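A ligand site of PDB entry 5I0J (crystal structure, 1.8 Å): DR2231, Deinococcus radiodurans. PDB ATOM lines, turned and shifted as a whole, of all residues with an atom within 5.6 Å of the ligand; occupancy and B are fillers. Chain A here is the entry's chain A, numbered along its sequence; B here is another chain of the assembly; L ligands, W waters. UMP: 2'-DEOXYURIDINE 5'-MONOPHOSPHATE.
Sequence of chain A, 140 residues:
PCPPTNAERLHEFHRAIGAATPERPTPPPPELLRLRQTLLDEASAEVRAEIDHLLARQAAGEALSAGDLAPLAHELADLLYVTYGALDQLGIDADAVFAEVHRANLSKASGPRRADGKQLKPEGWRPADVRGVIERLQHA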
ATOM      1  N   VAL A 101       4.071  21.025  29.273  1.00  0.00           N
ATOM      2  CA  VAL A 101       5.533  21.013  29.193  1.00  0.00           C
ATOM      3  C   VAL A 101       6.035  22.105  28.253  1.00  0.00           C
ATOM      4  O   VAL A 101       7.021  22.802  28.541  1.00  0.00           O
ATOM      5  CB  VAL A 101       6.038  19.626  28.765  1.00  0.00           C
ATOM      6  CG1 VAL A 101       7.541  19.650  28.427  1.00  0.00           C
ATOM      7  CG2 VAL A 101       5.759  18.596  29.867  1.00  0.00           C
ATOM      8  N   ASN A 105       8.500  25.312  28.830  1.00  0.00           N
ATOM      9  CA  ASN A 105       9.767  25.442  28.114  1.00  0.00           C
ATOM     10  C   ASN A 105       9.900  26.802  27.434  1.00  0.00           C
ATOM     11  O   ASN A 105      10.994  27.388  27.406  1.00  0.00           O
ATOM     12  CB  ASN A 105       9.922  24.292  27.112  1.00  0.00           C
ATOM     13  CG  ASN A 105      10.342  23.000  27.797  1.00  0.00           C
ATOM     14  OD1 ASN A 105      10.817  23.040  28.937  1.00  0.00           O
ATOM     15  ND2 ASN A 105      10.156  21.848  27.146  1.00  0.00           N
ATOM     16  N   LYS A 108      11.534  29.508  29.422  1.00  0.00           N
ATOM     17  CA  LYS A 108      12.978  29.457  29.654  1.00  0.00           C
ATOM     18  C   LYS A 108      13.755  30.420  28.770  1.00  0.00           C
ATOM     19  O   LYS A 108      14.986  30.505  28.919  1.00  0.00           O
ATOM     20  CB  LYS A 108      13.521  28.052  29.420  1.00  0.00           C
ATOM     21  CG  LYS A 108      12.829  26.998  30.257  1.00  0.00           C
ATOM     22  CD  LYS A 108      13.312  25.614  29.860  1.00  0.00           C
ATOM     23  CE  LYS A 108      12.754  24.582  30.856  1.00  0.00           C
ATOM     24  NZ  LYS A 108      13.237  23.221  30.547  1.00  0.00           N
ATOM     25  N   GLY A 117      25.120  24.141  24.180  1.00  0.00           N
ATOM     26  CA  GLY A 117      23.962  24.721  23.522  1.00  0.00           C
ATOM     27  C   GLY A 117      22.661  24.524  24.278  1.00  0.00           C
ATOM     28  O   GLY A 117      21.664  25.163  23.923  1.00  0.00           O
ATOM     29  N   LYS A 118      22.637  23.676  25.300  1.00  0.00           N
ATOM     30  CA  LYS A 118      21.393  23.428  26.023  1.00  0.00           C
ATOM     31  C   LYS A 118      20.839  24.714  26.653  1.00  0.00           C
ATOM     32  O   LYS A 118      21.569  25.474  27.297  1.00  0.00           O
ATOM     33  CB  LYS A 118      21.597  22.365  27.105  1.00  0.00           C
ATOM     34  CG  LYS A 118      20.286  22.042  27.827  1.00  0.00           C
ATOM     35  CD  LYS A 118      20.533  21.058  28.985  1.00  0.00           C
ATOM     36  CE  LYS A 118      19.227  20.678  29.679  1.00  0.00           C
ATOM     37  NZ  LYS A 118      19.472  19.643  30.739  1.00  0.00           N
ATOM     38  N   GLN A 119      19.553  24.948  26.437  1.00  0.00           N
ATOM     39  CA  GLN A 119      18.853  26.059  27.065  1.00  0.00           C
ATOM     40  C   GLN A 119      18.662  25.773  28.550  1.00  0.00           C
ATOM     41  O   GLN A 119      18.113  24.725  28.928  1.00  0.00           O
ATOM     42  CB  GLN A 119      17.517  26.290  26.375  1.00  0.00           C
ATOM     43  CG  GLN A 119      16.710  27.443  26.983  1.00  0.00           C
ATOM     44  CD  GLN A 119      17.457  28.770  26.876  1.00  0.00           C
ATOM     45  OE1 GLN A 119      17.835  29.192  25.772  1.00  0.00           O
ATOM     46  NE2 GLN A 119      17.697  29.421  28.006  1.00  0.00           N
ATOM     47  N   LEU A 120      19.078  26.698  29.395  1.00  0.00           N
ATOM     48  CA  LEU A 120      18.980  26.520  30.839  1.00  0.00           C
ATOM     49  C   LEU A 120      17.894  27.443  31.388  1.00  0.00           C
ATOM     50  O   LEU A 120      17.372  28.314  30.692  1.00  0.00           O
ATOM     51  CB  LEU A 120      20.325  26.780  31.522  1.00  0.00           C
ATOM     52  CG  LEU A 120      21.480  25.876  31.060  1.00  0.00           C
ATOM     53  CD1 LEU A 120      22.808  26.249  31.721  1.00  0.00           C
ATOM     54  CD2 LEU A 120      21.167  24.414  31.291  1.00  0.00           C
ATOM     55  N   LYS A 121      17.594  27.263  32.674  1.00  0.00           N
ATOM     56  CA  LYS A 121      16.438  27.919  33.268  1.00  0.00           C
ATOM     57  C   LYS A 121      16.815  29.270  33.869  1.00  0.00           C
ATOM     58  O   LYS A 121      17.801  29.367  34.610  1.00  0.00           O
ATOM     59  CB  LYS A 121      15.834  27.033  34.349  1.00  0.00           C
ATOM     60  CG  LYS A 121      15.177  25.777  33.773  1.00  0.00           C
ATOM     61  CD  LYS A 121      15.184  24.645  34.777  1.00  0.00           C
ATOM     62  CE  LYS A 121      14.733  23.331  34.130  1.00  0.00           C
ATOM     63  NZ  LYS A 121      14.864  22.200  35.084  1.00  0.00           N
ATOM     64  N   LEU B  10       7.711  22.729  18.792  1.00  0.00           N
ATOM     65  CA  LEU B  10       9.165  22.748  18.859  1.00  0.00           C
ATOM     66  C   LEU B  10       9.730  23.857  17.985  1.00  0.00           C
ATOM     67  O   LEU B  10      10.736  24.492  18.336  1.00  0.00           O
ATOM     68  CB  LEU B  10       9.762  21.407  18.426  1.00  0.00           C
ATOM     69  CG  LEU B  10      10.283  20.501  19.562  1.00  0.00           C
ATOM     70  CD1 LEU B  10      11.364  21.207  20.370  1.00  0.00           C
ATOM     71  CD2 LEU B  10       9.157  20.128  20.488  1.00  0.00           C
ATOM     72  N   PHE B  13       9.467  26.962  20.040  1.00  0.00           N
ATOM     73  CA  PHE B  13      10.460  26.973  21.099  1.00  0.00           C
ATOM     74  C   PHE B  13      11.846  27.341  20.560  1.00  0.00           C
ATOM     75  O   PHE B  13      12.535  28.207  21.105  1.00  0.00           O
ATOM     76  CB  PHE B  13      10.470  25.604  21.792  1.00  0.00           C
ATOM     77  CG  PHE B  13      11.576  25.429  22.791  1.00  0.00           C
ATOM     78  CD1 PHE B  13      11.560  26.087  24.006  1.00  0.00           C
ATOM     79  CD2 PHE B  13      12.622  24.562  22.531  1.00  0.00           C
ATOM     80  CE1 PHE B  13      12.573  25.896  24.935  1.00  0.00           C
ATOM     81  CE2 PHE B  13      13.641  24.365  23.444  1.00  0.00           C
ATOM     82  CZ  PHE B  13      13.612  25.027  24.654  1.00  0.00           C
ATOM     83  N   HIS B  14      12.247  26.726  19.451  1.00  0.00           N
ATOM     84  CA  HIS B  14      13.591  26.994  18.948  1.00  0.00           C
ATOM     85  C   HIS B  14      13.713  28.420  18.427  1.00  0.00           C
ATOM     86  O   HIS B  14      14.739  29.072  18.649  1.00  0.00           O
ATOM     87  CB  HIS B  14      13.959  25.967  17.893  1.00  0.00           C
ATOM     88  CG  HIS B  14      14.333  24.639  18.479  1.00  0.00           C
ATOM     89  ND1 HIS B  14      14.314  23.463  17.758  1.00  0.00           N
ATOM     90  CD2 HIS B  14      14.695  24.304  19.735  1.00  0.00           C
ATOM     91  CE1 HIS B  14      14.675  22.465  18.551  1.00  0.00           C
ATOM     92  NE2 HIS B  14      14.910  22.945  19.756  1.00  0.00           N
ATOM     93  N   ILE B  17      14.187  30.696  21.474  1.00  0.00           N
ATOM     94  CA  ILE B  17      15.468  30.630  22.187  1.00  0.00           C
ATOM     95  C   ILE B  17      16.651  30.849  21.260  1.00  0.00           C
ATOM     96  O   ILE B  17      17.799  30.819  21.734  1.00  0.00           O
ATOM     97  CB  ILE B  17      15.632  29.293  22.945  1.00  0.00           C
ATOM     98  CG1 ILE B  17      15.846  28.121  21.977  1.00  0.00           C
ATOM     99  CG2 ILE B  17      14.406  29.038  23.858  1.00  0.00           C
ATOM    100  CD1 ILE B  17      16.344  26.807  22.651  1.00  0.00           C
ATOM    101  N   LEU B  35      24.731  17.731  20.770  1.00  0.00           N
ATOM    102  CA  LEU B  35      23.725  18.238  21.696  1.00  0.00           C
ATOM    103  C   LEU B  35      22.456  17.381  21.658  1.00  0.00           C
ATOM    104  O   LEU B  35      21.890  17.059  22.707  1.00  0.00           O
ATOM    105  CB  LEU B  35      23.374  19.699  21.372  1.00  0.00           C
ATOM    106  CG  LEU B  35      22.207  20.246  22.256  1.00  0.00           C
ATOM    107  CD1 LEU B  35      22.585  20.272  23.762  1.00  0.00           C
ATOM    108  CD2 LEU B  35      21.765  21.649  21.799  1.00  0.00           C
ATOM    109  N   ARG B  36      21.995  17.022  20.461  1.00  0.00           N
ATOM    110  CA  ARG B  36      20.772  16.219  20.366  1.00  0.00           C
ATOM    111  C   ARG B  36      20.949  14.878  21.072  1.00  0.00           C
ATOM    112  O   ARG B  36      20.023  14.410  21.752  1.00  0.00           O
ATOM    113  CB  ARG B  36      20.397  15.993  18.903  1.00  0.00           C
ATOM    114  CG  ARG B  36      20.112  17.251  18.049  1.00  0.00           C
ATOM    115  CD  ARG B  36      19.423  18.404  18.788  1.00  0.00           C
ATOM    116  NE  ARG B  36      18.209  18.029  19.530  1.00  0.00           N
ATOM    117  CZ  ARG B  36      17.450  18.901  20.189  1.00  0.00           C
ATOM    118  NH1 ARG B  36      17.766  20.186  20.161  1.00  0.00           N
ATOM    119  NH2 ARG B  36      16.396  18.489  20.889  1.00  0.00           N
ATOM    120  N   LEU B  39      20.738  15.549  24.854  1.00  0.00           N
ATOM    121  CA  LEU B  39      19.376  15.811  25.307  1.00  0.00           C
ATOM    122  C   LEU B  39      18.545  14.522  25.319  1.00  0.00           C
ATOM    123  O   LEU B  39      17.721  14.321  26.230  1.00  0.00           O
ATOM    124  CB  LEU B  39      18.724  16.851  24.406  1.00  0.00           C
ATOM    125  CG  LEU B  39      19.292  18.281  24.538  1.00  0.00           C
ATOM    126  CD1 LEU B  39      18.561  19.240  23.608  1.00  0.00           C
ATOM    127  CD2 LEU B  39      19.227  18.777  25.991  1.00  0.00           C
ATOM    128  N   GLU B  42      19.742  12.457  28.385  1.00  0.00           N
ATOM    129  CA  GLU B  42      19.202  13.027  29.625  1.00  0.00           C
ATOM    130  C   GLU B  42      17.738  12.646  29.807  1.00  0.00           C
ATOM    131  O   GLU B  42      17.331  12.214  30.900  1.00  0.00           O
ATOM    132  CB  GLU B  42      19.352  14.555  29.611  1.00  0.00           C
ATOM    133  CG  GLU B  42      20.795  15.026  29.770  1.00  0.00           C
ATOM    134  CD  GLU B  42      20.981  16.555  29.710  1.00  0.00           C
ATOM    135  OE1 GLU B  42      19.984  17.279  29.478  1.00  0.00           O
ATOM    136  OE2 GLU B  42      22.113  17.030  29.931  1.00  0.00           O
ATOM    137  N   ALA B  77       6.915  13.025  28.173  1.00  0.00           N
ATOM    138  CA  ALA B  77       6.730  14.206  27.337  1.00  0.00           C
ATOM    139  C   ALA B  77       8.058  14.942  27.092  1.00  0.00           C
ATOM    140  O   ALA B  77       8.270  15.482  26.004  1.00  0.00           O
ATOM    141  CB  ALA B  77       5.702  15.140  27.960  1.00  0.00           C
ATOM    142  N   ASP B  78       8.946  14.993  28.089  1.00  0.00           N
ATOM    143  CA  ASP B  78      10.274  15.564  27.841  1.00  0.00           C
ATOM    144  C   ASP B  78      10.998  14.786  26.767  1.00  0.00           C
ATOM    145  O   ASP B  78      11.727  15.363  25.948  1.00  0.00           O
ATOM    146  CB  ASP B  78      11.120  15.559  29.123  1.00  0.00           C
ATOM    147  CG  ASP B  78      10.795  16.705  30.057  1.00  0.00           C
ATOM    148  OD1 ASP B  78      10.095  17.657  29.638  1.00  0.00           O
ATOM    149  OD2 ASP B  78      11.262  16.651  31.216  1.00  0.00           O
ATOM    150  N   TYR B  81       9.678  15.772  23.587  1.00  0.00           N
ATOM    151  CA  TYR B  81      10.104  17.132  23.290  1.00  0.00           C
ATOM    152  C   TYR B  81      11.478  17.156  22.630  1.00  0.00           C
ATOM    153  O   TYR B  81      11.666  17.848  21.631  1.00  0.00           O
ATOM    154  CB  TYR B  81      10.109  17.976  24.565  1.00  0.00           C
ATOM    155  CG  TYR B  81       9.836  19.437  24.318  1.00  0.00           C
ATOM    156  CD1 TYR B  81      10.864  20.312  23.991  1.00  0.00           C
ATOM    157  CD2 TYR B  81       8.540  19.947  24.396  1.00  0.00           C
ATOM    158  CE1 TYR B  81      10.609  21.649  23.758  1.00  0.00           C
ATOM    159  CE2 TYR B  81       8.273  21.276  24.150  1.00  0.00           C
ATOM    160  CZ  TYR B  81       9.310  22.130  23.827  1.00  0.00           C
ATOM    161  OH  TYR B  81       9.055  23.468  23.594  1.00  0.00           O
ATOM    162  N   VAL B  82      12.435  16.376  23.160  1.00  0.00           N
ATOM    163  CA  VAL B  82      13.781  16.411  22.590  1.00  0.00           C
ATOM    164  C   VAL B  82      13.905  15.510  21.367  1.00  0.00           C
ATOM    165  O   VAL B  82      14.852  15.674  20.589  1.00  0.00           O
ATOM    166  CB  VAL B  82      14.857  15.997  23.611  1.00  0.00           C
ATOM    167  CG1 VAL B  82      14.774  16.864  24.847  1.00  0.00           C
ATOM    168  CG2 VAL B  82      14.738  14.504  23.997  1.00  0.00           C
HETATM  169  N1  UMP L   1      14.706  21.411  26.438  1.00  0.00           N
HETATM  170  C2  UMP L   1      14.946  21.362  24.992  1.00  0.00           C
HETATM  171  N3  UMP L   1      16.195  21.963  24.448  1.00  0.00           N
HETATM  172  C4  UMP L   1      17.160  22.585  25.346  1.00  0.00           C
HETATM  173  C5  UMP L   1      16.901  22.613  26.807  1.00  0.00           C
HETATM  174  C6  UMP L   1      15.661  22.024  27.336  1.00  0.00           C
HETATM  175  O2  UMP L   1      14.144  20.857  24.260  1.00  0.00           O
HETATM  176  O4  UMP L   1      18.162  23.058  24.916  1.00  0.00           O
HETATM  177  C1' UMP L   1      13.468  20.861  26.986  1.00  0.00           C
HETATM  178  C2' UMP L   1      13.416  19.289  26.913  1.00  0.00           C
HETATM  179  C3' UMP L   1      12.637  18.961  28.178  1.00  0.00           C
HETATM  180  C4' UMP L   1      13.051  19.869  29.094  1.00  0.00           C
HETATM  181  O3' UMP L   1      11.192  19.148  27.881  1.00  0.00           O
HETATM  182  O4' UMP L   1      13.395  21.196  28.252  1.00  0.00           O
HETATM  183  C5' UMP L   1      14.301  19.419  29.799  1.00  0.00           C
HETATM  184  O5' UMP L   1      14.964  20.532  30.366  1.00  0.00           O
HETATM  185  P   UMP L   1      15.831  20.276  31.762  1.00  0.00           P
HETATM  186  OP1 UMP L   1      14.860  19.966  32.878  1.00  0.00           O
HETATM  187  OP2 UMP L   1      16.608  21.534  32.060  1.00  0.00           O
HETATM  188  OP3 UMP L   1      16.738  19.093  31.547  1.00  0.00           O
HETATM  189  O   HOH W   1      14.425  20.302  21.705  1.00  0.00           O
HETATM  190  O   HOH W   2      12.488  21.364  32.364  1.00  0.00           O
HETATM  191  O   HOH W   3      16.615  16.515  32.585  1.00  0.00           O
HETATM  192  O   HOH W   4      18.954  24.212  22.291  1.00  0.00           O
HETATM  193  O   HOH W   5      17.291  17.730  28.929  1.00  0.00           O
HETATM  194  O   HOH W   6      14.562  18.263  35.241  1.00  0.00           O
HETATM  195  O   HOH W   7      16.765  22.274  21.917  1.00  0.00           O
HETATM  196  O   HOH W   8      18.420  22.415  33.694  1.00  0.00           O
HETATM  197  O   HOH W   9      16.079  23.663  30.416  1.00  0.00           O
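Water W7 lies within hydrogen-bond range of a nitrogen (N3) of the ligand (2.6 Å), the guanidinium group (NH1) of Arg 36 of chain B (2.9 Å) and a ring nitrogen (NE2) of His 14 of chain B (2.9 Å).
Water W1 lies within hydrogen-bond range of O2 of the ligand (2.6 Å), NH2 of Arg 36 of chain B (2.8 Å) and NE2 of His 14 of chain B (3.3 Å).
Water W9 lies within hydrogen-bond range of the backbone carbonyl oxygen (O) of Gln 119, an oxygen (OP2) of the ligand and the side-chain amino group (NZ) of Lys 108.
Water W2 lies within hydrogen-bond range of NZ of Lys 108 and OP1 of the ligand.
Water W4 lies within hydrogen-bond range of an oxygen (O4) of the ligand (3.0 Å) and the backbone carbonyl oxygen of Gly 117 (3.3 Å).
Water W5 lies within hydrogen-bond range of OE1 of Glu 42 of chain B (2.8 Å), OP3 of the ligand (3.0 Å) and NZ of Lys 118 (3.4 Å).
The side-chain amino group of Lys 118 lies within salt-bridge range of the side-chain carboxylate of Glu 42 of chain B.
The backbone carbonyl oxygen of Val 82 of chain B lies within hydrogen-bond range of the guanidinium group of Arg 36 of chain B, 3.2 Å away.
The side-chain amide oxygen (OD1) of Asn 105 sits at hydrogen-bond distance from the side-chain amino group (NZ) of Lys 108 (2.9 Å).
O of Lys 108 sits at hydrogen-bond distance from NE2 of Gln 119 (3.1 Å).
An oxygen (O4') of the ligand sits at hydrogen-bond distance from the side-chain amino group of Lys 108 (3.1 Å).
The side-chain carboxylate of Asp 78 of chain B sits at hydrogen-bond distance from an oxygen (O3') of the ligand (2.6 Å).
An oxygen (OP3) of the ligand lies within salt-bridge range of the side-chain amino group (NZ) of Lys 118 (2.9 Å).
NZ of Lys 121 lies within salt-bridge range of OP1 of the ligand (3.1 Å).
The backbone NH of Gln 119 lies within hydrogen-bond range of an oxygen (O4) of the ligand (2.8 Å).
O3' of the ligand lies within hydrogen-bond range of ND2 of Asn 105 (3.0 Å).
Merely in contact with the ligand: Tyr 81 of chain B (3.3 Å), Val 82 of chain B (3.5 Å), Phe 13 of chain B (3.6 Å), Leu 39 of chain B (3.7 Å) and Val 101 (3.7 Å).
Hydrophobic or aromatic side chains that line the ligand: Val 101, Phe 13 of chain B, Leu 39 of chain B, Tyr 81 of chain B and Val 82 of chain B.
Within 4 Å of the ligand: Val 101, Asn 105, Lys 108, Lys 118, Gln 119, Lys 121, Phe 13 of chain B, Leu 39 of chain B, Asp 78 of chain B, Tyr 81 of chain B and Val 82 of chain B.
The nearest printed residue that does not touch the ligand is Gly 117 (4.2 Å).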
